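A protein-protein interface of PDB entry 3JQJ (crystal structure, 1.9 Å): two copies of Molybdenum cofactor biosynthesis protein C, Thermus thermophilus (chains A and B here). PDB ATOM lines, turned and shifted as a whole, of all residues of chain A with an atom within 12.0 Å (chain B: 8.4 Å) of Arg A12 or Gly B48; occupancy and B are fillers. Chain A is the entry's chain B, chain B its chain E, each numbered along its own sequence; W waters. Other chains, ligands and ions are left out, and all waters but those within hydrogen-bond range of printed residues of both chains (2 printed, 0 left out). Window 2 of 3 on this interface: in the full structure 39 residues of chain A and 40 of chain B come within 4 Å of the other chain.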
ATOM      1  N   GLY A   9       3.564 -21.316 -13.206  1.00  0.00           N
ATOM      2  CA  GLY A   9       4.928 -21.908 -13.113  1.00  0.00           C
ATOM      3  C   GLY A   9       4.930 -23.425 -13.129  1.00  0.00           C
ATOM      4  O   GLY A   9       5.961 -24.045 -13.393  1.00  0.00           O
ATOM      5  N   ARG A  10       3.783 -24.034 -12.840  1.00  0.00           N
ATOM      6  CA  ARG A  10       3.702 -25.490 -12.839  1.00  0.00           C
ATOM      7  C   ARG A  10       3.385 -25.986 -14.245  1.00  0.00           C
ATOM      8  O   ARG A  10       2.828 -25.253 -15.060  1.00  0.00           O
ATOM      9  CB  ARG A  10       2.635 -25.982 -11.848  1.00  0.00           C
ATOM     10  CG  ARG A  10       1.193 -25.800 -12.291  1.00  0.00           C
ATOM     11  CD  ARG A  10       0.256 -26.598 -11.386  1.00  0.00           C
ATOM     12  NE  ARG A  10      -1.113 -26.637 -11.894  1.00  0.00           N
ATOM     13  CZ  ARG A  10      -2.010 -25.674 -11.721  1.00  0.00           C
ATOM     14  NH1 ARG A  10      -1.694 -24.580 -11.041  1.00  0.00           N
ATOM     15  NH2 ARG A  10      -3.226 -25.803 -12.233  1.00  0.00           N
ATOM     16  N   PRO A  11       3.742 -27.242 -14.549  1.00  0.00           N
ATOM     17  CA  PRO A  11       3.495 -27.832 -15.870  1.00  0.00           C
ATOM     18  C   PRO A  11       2.014 -27.916 -16.240  1.00  0.00           C
ATOM     19  O   PRO A  11       1.162 -28.121 -15.377  1.00  0.00           O
ATOM     20  CB  PRO A  11       4.115 -29.223 -15.751  1.00  0.00           C
ATOM     21  CG  PRO A  11       5.151 -29.066 -14.676  1.00  0.00           C
ATOM     22  CD  PRO A  11       4.441 -28.200 -13.674  1.00  0.00           C
ATOM     23  N   ARG A  12       1.722 -27.774 -17.533  1.00  0.00           N
ATOM     24  CA  ARG A  12       0.353 -27.853 -18.035  1.00  0.00           C
ATOM     25  C   ARG A  12       0.333 -28.070 -19.543  1.00  0.00           C
ATOM     26  O   ARG A  12       1.249 -27.650 -20.247  1.00  0.00           O
ATOM     27  CB  ARG A  12      -0.408 -26.561 -17.736  1.00  0.00           C
ATOM     28  CG  ARG A  12       0.131 -25.354 -18.494  1.00  0.00           C
ATOM     29  CD  ARG A  12      -0.851 -24.192 -18.485  1.00  0.00           C
ATOM     30  NE  ARG A  12      -1.306 -23.869 -17.135  1.00  0.00           N
ATOM     31  CZ  ARG A  12      -0.502 -23.522 -16.135  1.00  0.00           C
ATOM     32  NH1 ARG A  12       0.808 -23.446 -16.326  1.00  0.00           N
ATOM     33  NH2 ARG A  12      -1.012 -23.253 -14.940  1.00  0.00           N
ATOM     34  N   MET A  13      -0.708 -28.734 -20.034  1.00  0.00           N
ATOM     35  CA  MET A  13      -0.858 -28.937 -21.468  1.00  0.00           C
ATOM     36  C   MET A  13      -1.730 -27.765 -21.895  1.00  0.00           C
ATOM     37  O   MET A  13      -2.942 -27.774 -21.671  1.00  0.00           O
ATOM     38  CB  MET A  13      -1.580 -30.248 -21.780  1.00  0.00           C
ATOM     39  CG  MET A  13      -1.667 -30.544 -23.267  1.00  0.00           C
ATOM     40  SD  MET A  13      -2.746 -31.929 -23.661  1.00  0.00           S
ATOM     41  CE  MET A  13      -1.830 -33.272 -22.925  1.00  0.00           C
ATOM     42  N   VAL A  14      -1.102 -26.754 -22.486  1.00  0.00           N
ATOM     43  CA  VAL A  14      -1.797 -25.552 -22.931  1.00  0.00           C
ATOM     44  C   VAL A  14      -3.176 -25.831 -23.513  1.00  0.00           C
ATOM     45  O   VAL A  14      -3.336 -26.676 -24.391  1.00  0.00           O
ATOM     46  CB  VAL A  14      -0.971 -24.781 -23.976  1.00  0.00           C
ATOM     47  CG1 VAL A  14      -1.730 -23.537 -24.420  1.00  0.00           C
ATOM     48  CG2 VAL A  14       0.376 -24.397 -23.387  1.00  0.00           C
ATOM     49  N   ASP A  15      -4.164 -25.103 -23.003  1.00  0.00           N
ATOM     50  CA  ASP A  15      -5.550 -25.237 -23.435  1.00  0.00           C
ATOM     51  C   ASP A  15      -5.757 -24.574 -24.792  1.00  0.00           C
ATOM     52  O   ASP A  15      -5.626 -23.359 -24.925  1.00  0.00           O
ATOM     53  CB  ASP A  15      -6.469 -24.599 -22.388  1.00  0.00           C
ATOM     54  CG  ASP A  15      -7.941 -24.768 -22.712  1.00  0.00           C
ATOM     55  OD1 ASP A  15      -8.772 -24.254 -21.936  1.00  0.00           O
ATOM     56  OD2 ASP A  15      -8.270 -25.411 -23.730  1.00  0.00           O
ATOM     57  N   VAL A  16      -6.078 -25.380 -25.799  1.00  0.00           N
ATOM     58  CA  VAL A  16      -6.300 -24.868 -27.147  1.00  0.00           C
ATOM     59  C   VAL A  16      -7.664 -25.314 -27.650  1.00  0.00           C
ATOM     60  O   VAL A  16      -7.915 -25.353 -28.854  1.00  0.00           O
ATOM     61  CB  VAL A  16      -5.216 -25.385 -28.115  1.00  0.00           C
ATOM     62  CG1 VAL A  16      -3.848 -24.936 -27.634  1.00  0.00           C
ATOM     63  CG2 VAL A  16      -5.275 -26.906 -28.210  1.00  0.00           C
ATOM     64  N   THR A  17      -8.544 -25.633 -26.706  1.00  0.00           N
ATOM     65  CA  THR A  17      -9.890 -26.108 -27.006  1.00  0.00           C
ATOM     66  C   THR A  17     -10.699 -25.208 -27.935  1.00  0.00           C
ATOM     67  O   THR A  17     -11.369 -25.698 -28.843  1.00  0.00           O
ATOM     68  CB  THR A  17     -10.701 -26.309 -25.703  1.00  0.00           C
ATOM     69  OG1 THR A  17      -9.947 -27.113 -24.789  1.00  0.00           O
ATOM     70  CG2 THR A  17     -12.019 -27.012 -26.000  1.00  0.00           C
ATOM     71  N   ALA A  68       3.630 -37.752 -28.606  1.00  0.00           N
ATOM     72  CA  ALA A  68       2.874 -37.345 -27.423  1.00  0.00           C
ATOM     73  C   ALA A  68       3.196 -38.219 -26.214  1.00  0.00           C
ATOM     74  O   ALA A  68       3.043 -37.793 -25.072  1.00  0.00           O
ATOM     75  CB  ALA A  68       1.374 -37.387 -27.713  1.00  0.00           C
ATOM     76  N   ILE A  71       6.925 -36.710 -25.099  1.00  0.00           N
ATOM     77  CA  ILE A  71       6.991 -35.317 -24.672  1.00  0.00           C
ATOM     78  C   ILE A  71       5.801 -35.022 -23.754  1.00  0.00           C
ATOM     79  O   ILE A  71       4.669 -34.872 -24.213  1.00  0.00           O
ATOM     80  CB  ILE A  71       6.961 -34.373 -25.900  1.00  0.00           C
ATOM     81  CG1 ILE A  71       7.956 -34.861 -26.962  1.00  0.00           C
ATOM     82  CG2 ILE A  71       7.291 -32.956 -25.475  1.00  0.00           C
ATOM     83  CD1 ILE A  71       9.405 -35.014 -26.466  1.00  0.00           C
ATOM     84  N   PRO A  72       6.055 -34.903 -22.442  1.00  0.00           N
ATOM     85  CA  PRO A  72       5.037 -34.640 -21.416  1.00  0.00           C
ATOM     86  C   PRO A  72       3.866 -33.715 -21.739  1.00  0.00           C
ATOM     87  O   PRO A  72       2.706 -34.126 -21.652  1.00  0.00           O
ATOM     88  CB  PRO A  72       5.866 -34.132 -20.232  1.00  0.00           C
ATOM     89  CG  PRO A  72       7.131 -34.912 -20.366  1.00  0.00           C
ATOM     90  CD  PRO A  72       7.409 -34.810 -21.861  1.00  0.00           C
ATOM     91  N   LEU A  73       4.154 -32.475 -22.115  1.00  0.00           N
ATOM     92  CA  LEU A  73       3.094 -31.513 -22.385  1.00  0.00           C
ATOM     93  C   LEU A  73       2.601 -31.436 -23.823  1.00  0.00           C
ATOM     94  O   LEU A  73       1.838 -30.538 -24.178  1.00  0.00           O
ATOM     95  CB  LEU A  73       3.540 -30.131 -21.914  1.00  0.00           C
ATOM     96  CG  LEU A  73       4.124 -30.156 -20.494  1.00  0.00           C
ATOM     97  CD1 LEU A  73       4.405 -28.733 -20.049  1.00  0.00           C
ATOM     98  CD2 LEU A  73       3.153 -30.840 -19.529  1.00  0.00           C
ATOM     99  N   CYS A  74       3.033 -32.383 -24.646  1.00  0.00           N
ATOM    100  CA  CYS A  74       2.630 -32.430 -26.047  1.00  0.00           C
ATOM    101  C   CYS A  74       1.167 -32.864 -26.154  1.00  0.00           C
ATOM    102  O   CYS A  74       0.713 -33.731 -25.404  1.00  0.00           O
ATOM    103  CB  CYS A  74       3.528 -33.416 -26.800  1.00  0.00           C
ATOM    104  SG  CYS A  74       3.299 -33.459 -28.581  1.00  0.00           S
ATOM    105  N   HIS A  75       0.426 -32.259 -27.079  1.00  0.00           N
ATOM    106  CA  HIS A  75      -0.980 -32.609 -27.260  1.00  0.00           C
ATOM    107  C   HIS A  75      -1.139 -33.856 -28.116  1.00  0.00           C
ATOM    108  O   HIS A  75      -0.462 -34.015 -29.135  1.00  0.00           O
ATOM    109  CB  HIS A  75      -1.760 -31.480 -27.949  1.00  0.00           C
ATOM    110  CG  HIS A  75      -1.826 -30.206 -27.168  1.00  0.00           C
ATOM    111  ND1 HIS A  75      -0.771 -29.322 -27.092  1.00  0.00           N
ATOM    112  CD2 HIS A  75      -2.832 -29.651 -26.451  1.00  0.00           C
ATOM    113  CE1 HIS A  75      -1.126 -28.278 -26.365  1.00  0.00           C
ATOM    114  NE2 HIS A  75      -2.372 -28.454 -25.964  1.00  0.00           N
ATOM    115  N   PRO A  76      -2.027 -34.771 -27.705  1.00  0.00           N
ATOM    116  CA  PRO A  76      -2.219 -35.977 -28.512  1.00  0.00           C
ATOM    117  C   PRO A  76      -3.045 -35.516 -29.706  1.00  0.00           C
ATOM    118  O   PRO A  76      -4.045 -34.816 -29.534  1.00  0.00           O
ATOM    119  CB  PRO A  76      -3.028 -36.892 -27.594  1.00  0.00           C
ATOM    120  CG  PRO A  76      -2.701 -36.391 -26.212  1.00  0.00           C
ATOM    121  CD  PRO A  76      -2.694 -34.898 -26.400  1.00  0.00           C
ATOM    122  N   THR A 107      -3.036 -27.232 -32.711  1.00  0.00           N
ATOM    123  CA  THR A 107      -1.647 -26.948 -32.350  1.00  0.00           C
ATOM    124  C   THR A 107      -0.698 -27.532 -33.399  1.00  0.00           C
ATOM    125  O   THR A 107      -1.045 -28.494 -34.088  1.00  0.00           O
ATOM    126  CB  THR A 107      -1.289 -27.521 -30.961  1.00  0.00           C
ATOM    127  OG1 THR A 107      -1.455 -28.943 -30.967  1.00  0.00           O
ATOM    128  CG2 THR A 107      -2.187 -26.918 -29.894  1.00  0.00           C
ATOM    129  N   MET A 111       6.973 -30.672 -32.761  1.00  0.00           N
ATOM    130  CA  MET A 111       7.526 -31.721 -31.914  1.00  0.00           C
ATOM    131  C   MET A 111       7.583 -33.057 -32.632  1.00  0.00           C
ATOM    132  O   MET A 111       8.548 -33.804 -32.475  1.00  0.00           O
ATOM    133  CB  MET A 111       6.726 -31.866 -30.613  1.00  0.00           C
ATOM    134  CG  MET A 111       6.931 -30.720 -29.636  1.00  0.00           C
ATOM    135  SD  MET A 111       8.666 -30.212 -29.552  1.00  0.00           S
ATOM    136  CE  MET A 111       9.452 -31.723 -29.043  1.00  0.00           C
ATOM    137  N   ALA B  41      13.432 -16.455 -21.042  1.00  0.00           N
ATOM    138  CA  ALA B  41      12.216 -17.143 -20.625  1.00  0.00           C
ATOM    139  C   ALA B  41      12.548 -18.197 -19.577  1.00  0.00           C
ATOM    140  O   ALA B  41      11.870 -18.308 -18.553  1.00  0.00           O
ATOM    141  CB  ALA B  41      11.542 -17.793 -21.832  1.00  0.00           C
ATOM    142  N   LYS B  44      12.971 -16.840 -16.149  1.00  0.00           N
ATOM    143  CA  LYS B  44      11.725 -16.353 -15.568  1.00  0.00           C
ATOM    144  C   LYS B  44      10.724 -17.460 -15.241  1.00  0.00           C
ATOM    145  O   LYS B  44       9.604 -17.181 -14.810  1.00  0.00           O
ATOM    146  CB  LYS B  44      11.083 -15.323 -16.501  1.00  0.00           C
ATOM    147  CG  LYS B  44      11.736 -13.954 -16.408  1.00  0.00           C
ATOM    148  CD  LYS B  44      11.518 -13.121 -17.660  1.00  0.00           C
ATOM    149  CE  LYS B  44      10.049 -12.856 -17.935  1.00  0.00           C
ATOM    150  NZ  LYS B  44       9.883 -12.024 -19.161  1.00  0.00           N
ATOM    151  N   GLY B  45      11.129 -18.713 -15.446  1.00  0.00           N
ATOM    152  CA  GLY B  45      10.249 -19.829 -15.140  1.00  0.00           C
ATOM    153  C   GLY B  45       9.659 -20.551 -16.336  1.00  0.00           C
ATOM    154  O   GLY B  45       8.908 -21.516 -16.174  1.00  0.00           O
ATOM    155  N   GLY B  46       9.992 -20.093 -17.537  1.00  0.00           N
ATOM    156  CA  GLY B  46       9.473 -20.728 -18.735  1.00  0.00           C
ATOM    157  C   GLY B  46       8.613 -19.792 -19.555  1.00  0.00           C
ATOM    158  O   GLY B  46       8.674 -18.573 -19.385  1.00  0.00           O
ATOM    159  N   VAL B  47       7.799 -20.361 -20.440  1.00  0.00           N
ATOM    160  CA  VAL B  47       6.927 -19.575 -21.307  1.00  0.00           C
ATOM    161  C   VAL B  47       5.472 -19.619 -20.846  1.00  0.00           C
ATOM    162  O   VAL B  47       4.608 -18.954 -21.420  1.00  0.00           O
ATOM    163  CB  VAL B  47       6.998 -20.091 -22.762  1.00  0.00           C
ATOM    164  CG1 VAL B  47       6.423 -21.497 -22.845  1.00  0.00           C
ATOM    165  CG2 VAL B  47       6.253 -19.145 -23.692  1.00  0.00           C
ATOM    166  N   GLY B  48       5.205 -20.405 -19.807  1.00  0.00           N
ATOM    167  CA  GLY B  48       3.852 -20.521 -19.298  1.00  0.00           C
ATOM    168  C   GLY B  48       3.407 -21.970 -19.245  1.00  0.00           C
ATOM    169  O   GLY B  48       2.289 -22.271 -18.829  1.00  0.00           O
ATOM    170  N   LYS B  49       4.294 -22.867 -19.671  1.00  0.00           N
ATOM    171  CA  LYS B  49       4.019 -24.299 -19.682  1.00  0.00           C
ATOM    172  C   LYS B  49       4.682 -24.968 -18.483  1.00  0.00           C
ATOM    173  O   LYS B  49       4.493 -26.161 -18.248  1.00  0.00           O
ATOM    174  CB  LYS B  49       4.554 -24.935 -20.971  1.00  0.00           C
ATOM    175  CG  LYS B  49       3.940 -24.386 -22.250  1.00  0.00           C
ATOM    176  CD  LYS B  49       4.559 -25.028 -23.494  1.00  0.00           C
ATOM    177  CE  LYS B  49       4.377 -26.541 -23.496  1.00  0.00           C
ATOM    178  NZ  LYS B  49       4.895 -27.184 -24.736  1.00  0.00           N
ATOM    179  N   GLY B  50       5.467 -24.194 -17.739  1.00  0.00           N
ATOM    180  CA  GLY B  50       6.150 -24.728 -16.575  1.00  0.00           C
ATOM    181  C   GLY B  50       7.664 -24.675 -16.687  1.00  0.00           C
ATOM    182  O   GLY B  50       8.203 -24.211 -17.692  1.00  0.00           O
ATOM    183  N   ASP B  51       8.342 -25.162 -15.651  1.00  0.00           N
ATOM    184  CA  ASP B  51       9.804 -25.189 -15.590  1.00  0.00           C
ATOM    185  C   ASP B  51      10.375 -26.150 -16.636  1.00  0.00           C
ATOM    186  O   ASP B  51      10.234 -27.366 -16.516  1.00  0.00           O
ATOM    187  CB  ASP B  51      10.252 -25.639 -14.196  1.00  0.00           C
ATOM    188  CG  ASP B  51      11.758 -25.544 -14.000  1.00  0.00           C
ATOM    189  OD1 ASP B  51      12.515 -25.927 -14.920  1.00  0.00           O
ATOM    190  OD2 ASP B  51      12.182 -25.098 -12.914  1.00  0.00           O
ATOM    191  N   PRO B  52      11.041 -25.611 -17.669  1.00  0.00           N
ATOM    192  CA  PRO B  52      11.641 -26.403 -18.748  1.00  0.00           C
ATOM    193  C   PRO B  52      12.572 -27.533 -18.296  1.00  0.00           C
ATOM    194  O   PRO B  52      12.458 -28.667 -18.764  1.00  0.00           O
ATOM    195  CB  PRO B  52      12.376 -25.347 -19.570  1.00  0.00           C
ATOM    196  CG  PRO B  52      11.497 -24.146 -19.417  1.00  0.00           C
ATOM    197  CD  PRO B  52      11.201 -24.169 -17.934  1.00  0.00           C
ATOM    198  N   VAL B  55      10.678 -30.490 -16.163  1.00  0.00           N
ATOM    199  CA  VAL B  55       9.905 -31.392 -17.018  1.00  0.00           C
ATOM    200  C   VAL B  55      10.786 -32.262 -17.910  1.00  0.00           C
ATOM    201  O   VAL B  55      10.504 -33.446 -18.115  1.00  0.00           O
ATOM    202  CB  VAL B  55       8.924 -30.606 -17.910  1.00  0.00           C
ATOM    203  CG1 VAL B  55       8.131 -31.568 -18.794  1.00  0.00           C
ATOM    204  CG2 VAL B  55       7.976 -29.792 -17.041  1.00  0.00           C
ATOM    205  N   ASP B 126      10.508 -28.315 -26.511  1.00  0.00           N
ATOM    206  CA  ASP B 126       9.059 -28.154 -26.406  1.00  0.00           C
ATOM    207  C   ASP B 126       8.678 -27.109 -25.360  1.00  0.00           C
ATOM    208  O   ASP B 126       7.754 -26.322 -25.563  1.00  0.00           O
ATOM    209  CB  ASP B 126       8.407 -29.483 -26.037  1.00  0.00           C
ATOM    210  CG  ASP B 126       6.899 -29.377 -25.923  1.00  0.00           C
ATOM    211  OD1 ASP B 126       6.251 -29.033 -26.934  1.00  0.00           O
ATOM    212  OD2 ASP B 126       6.365 -29.637 -24.828  1.00  0.00           O
ATOM    213  N   MET B 127       9.405 -27.106 -24.246  1.00  0.00           N
ATOM    214  CA  MET B 127       9.138 -26.183 -23.152  1.00  0.00           C
ATOM    215  C   MET B 127       9.559 -24.745 -23.448  1.00  0.00           C
ATOM    216  O   MET B 127       9.155 -23.824 -22.734  1.00  0.00           O
ATOM    217  CB  MET B 127       9.844 -26.660 -21.879  1.00  0.00           C
ATOM    218  CG  MET B 127       9.443 -28.048 -21.400  1.00  0.00           C
ATOM    219  SD  MET B 127       7.709 -28.154 -20.935  1.00  0.00           S
ATOM    220  CE  MET B 127       7.707 -27.190 -19.408  1.00  0.00           C
ATOM    221  N   LEU B 128      10.358 -24.544 -24.495  1.00  0.00           N
ATOM    222  CA  LEU B 128      10.824 -23.200 -24.835  1.00  0.00           C
ATOM    223  C   LEU B 128      10.588 -22.735 -26.273  1.00  0.00           C
ATOM    224  O   LEU B 128      10.762 -21.551 -26.571  1.00  0.00           O
ATOM    225  CB  LEU B 128      12.325 -23.075 -24.521  1.00  0.00           C
ATOM    226  CG  LEU B 128      12.762 -23.143 -23.052  1.00  0.00           C
ATOM    227  CD1 LEU B 128      14.281 -23.200 -22.960  1.00  0.00           C
ATOM    228  CD2 LEU B 128      12.231 -21.929 -22.300  1.00  0.00           C
ATOM    229  N   ALA B 130       8.153 -21.848 -27.797  1.00  0.00           N
ATOM    230  CA  ALA B 130       7.224 -20.732 -27.898  1.00  0.00           C
ATOM    231  C   ALA B 130       8.031 -19.437 -27.949  1.00  0.00           C
ATOM    232  O   ALA B 130       7.610 -18.453 -28.553  1.00  0.00           O
ATOM    233  CB  ALA B 130       6.283 -20.724 -26.701  1.00  0.00           C
HETATM  234  O   HOH W   1       6.914 -26.404 -13.219  1.00  0.00           O
HETATM  235  O   HOH W   2       6.917 -31.129 -22.434  1.00  0.00           O
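The backbone carbonyl oxygen of Gly A9 sits at hydrogen-bond distance from the backbone NH of Asp B51 (3.5 Å).
The backbone NH (N) of Arg A12 is in hydrogen-bond range of the backbone carbonyl oxygen (O) of Lys B49.
The backbone carbonyl oxygen (O) of Gly B48 is in hydrogen-bond range of the guanidinium group (NH1) of Arg A12 (3.1 Å).
OD1 of Asp B126 lies close to SD of Met A111, 3.8 Å away.
The backbone carbonyl oxygen (O) of Val A14 lies within hydrogen-bond range of a ring nitrogen (NE2) of His A75, at 2.6 Å.
NZ of Lys B49 lies within salt-bridge range of OD2 of Asp B126, 2.9 Å away.
The backbone carbonyl oxygen (O) of Arg A10 lies within hydrogen-bond range of the guanidinium group (NH1) of Arg A12, at 3.0 Å.
Among the printed residues, pairs that only touch across the chains: Gly A9 with Gly B50, Arg A10 with Lys B49, Arg A10 with Gly B50, Pro A11 with Lys B49, Pro A11 with Val B55, Val A14 with Lys B49, Ile A71 with Asp B126, Pro A72 with Val B55, Leu A73 with Lys B49 and Leu A73 with Met B127.
Of the printed residues of chain B, Gly A9 touches Gly B50 and Asp B51.
Arg A12 touches two residues of chain B.
No residue of chain A comes within 4 Å of Gly B46.
Gly B48 touches one residue of chain A.
Lys B49 touches just these residues of chain A: Arg A10, Pro A11, Arg A12, Val A14 and Leu A73.
Of chain A, only Gly A9 and Arg A10 come within 4 Å of Gly B50.
Of the printed residues of chain A, Asp B51 touches Gly A9.
Printed residues of chain A within 4 Å of Asp B126: Ile A71 and Met A111.
The nearest residue of chain B that does not touch Arg A12 is Gly B50 (4.9 Å).
Hydrophobic or aromatic side chains of chain A within 4 Å of the printed part of chain B: Pro A11, Val A14, Ile A71, Pro A72, Leu A73 and Met A111.
Among the printed residues, 14 pairs touch across the chains.
Among the printed residues, no Asp or Glu carboxylate lies within 4 Å of a Lys or Arg side-chain nitrogen of the other chain.
No position is printed for both chains.
Water W1 lies within hydrogen-bond range of O of Gly A9 (2.6 Å) and N of Asp B51 (3.1 Å).
Water W2 lies within hydrogen-bond range of the side-chain carboxylate of Asp B126 (2.9 Å), the backbone NH of Leu A73 (3.1 Å) and the side-chain sulfur of Met B127 (3.4 Å).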
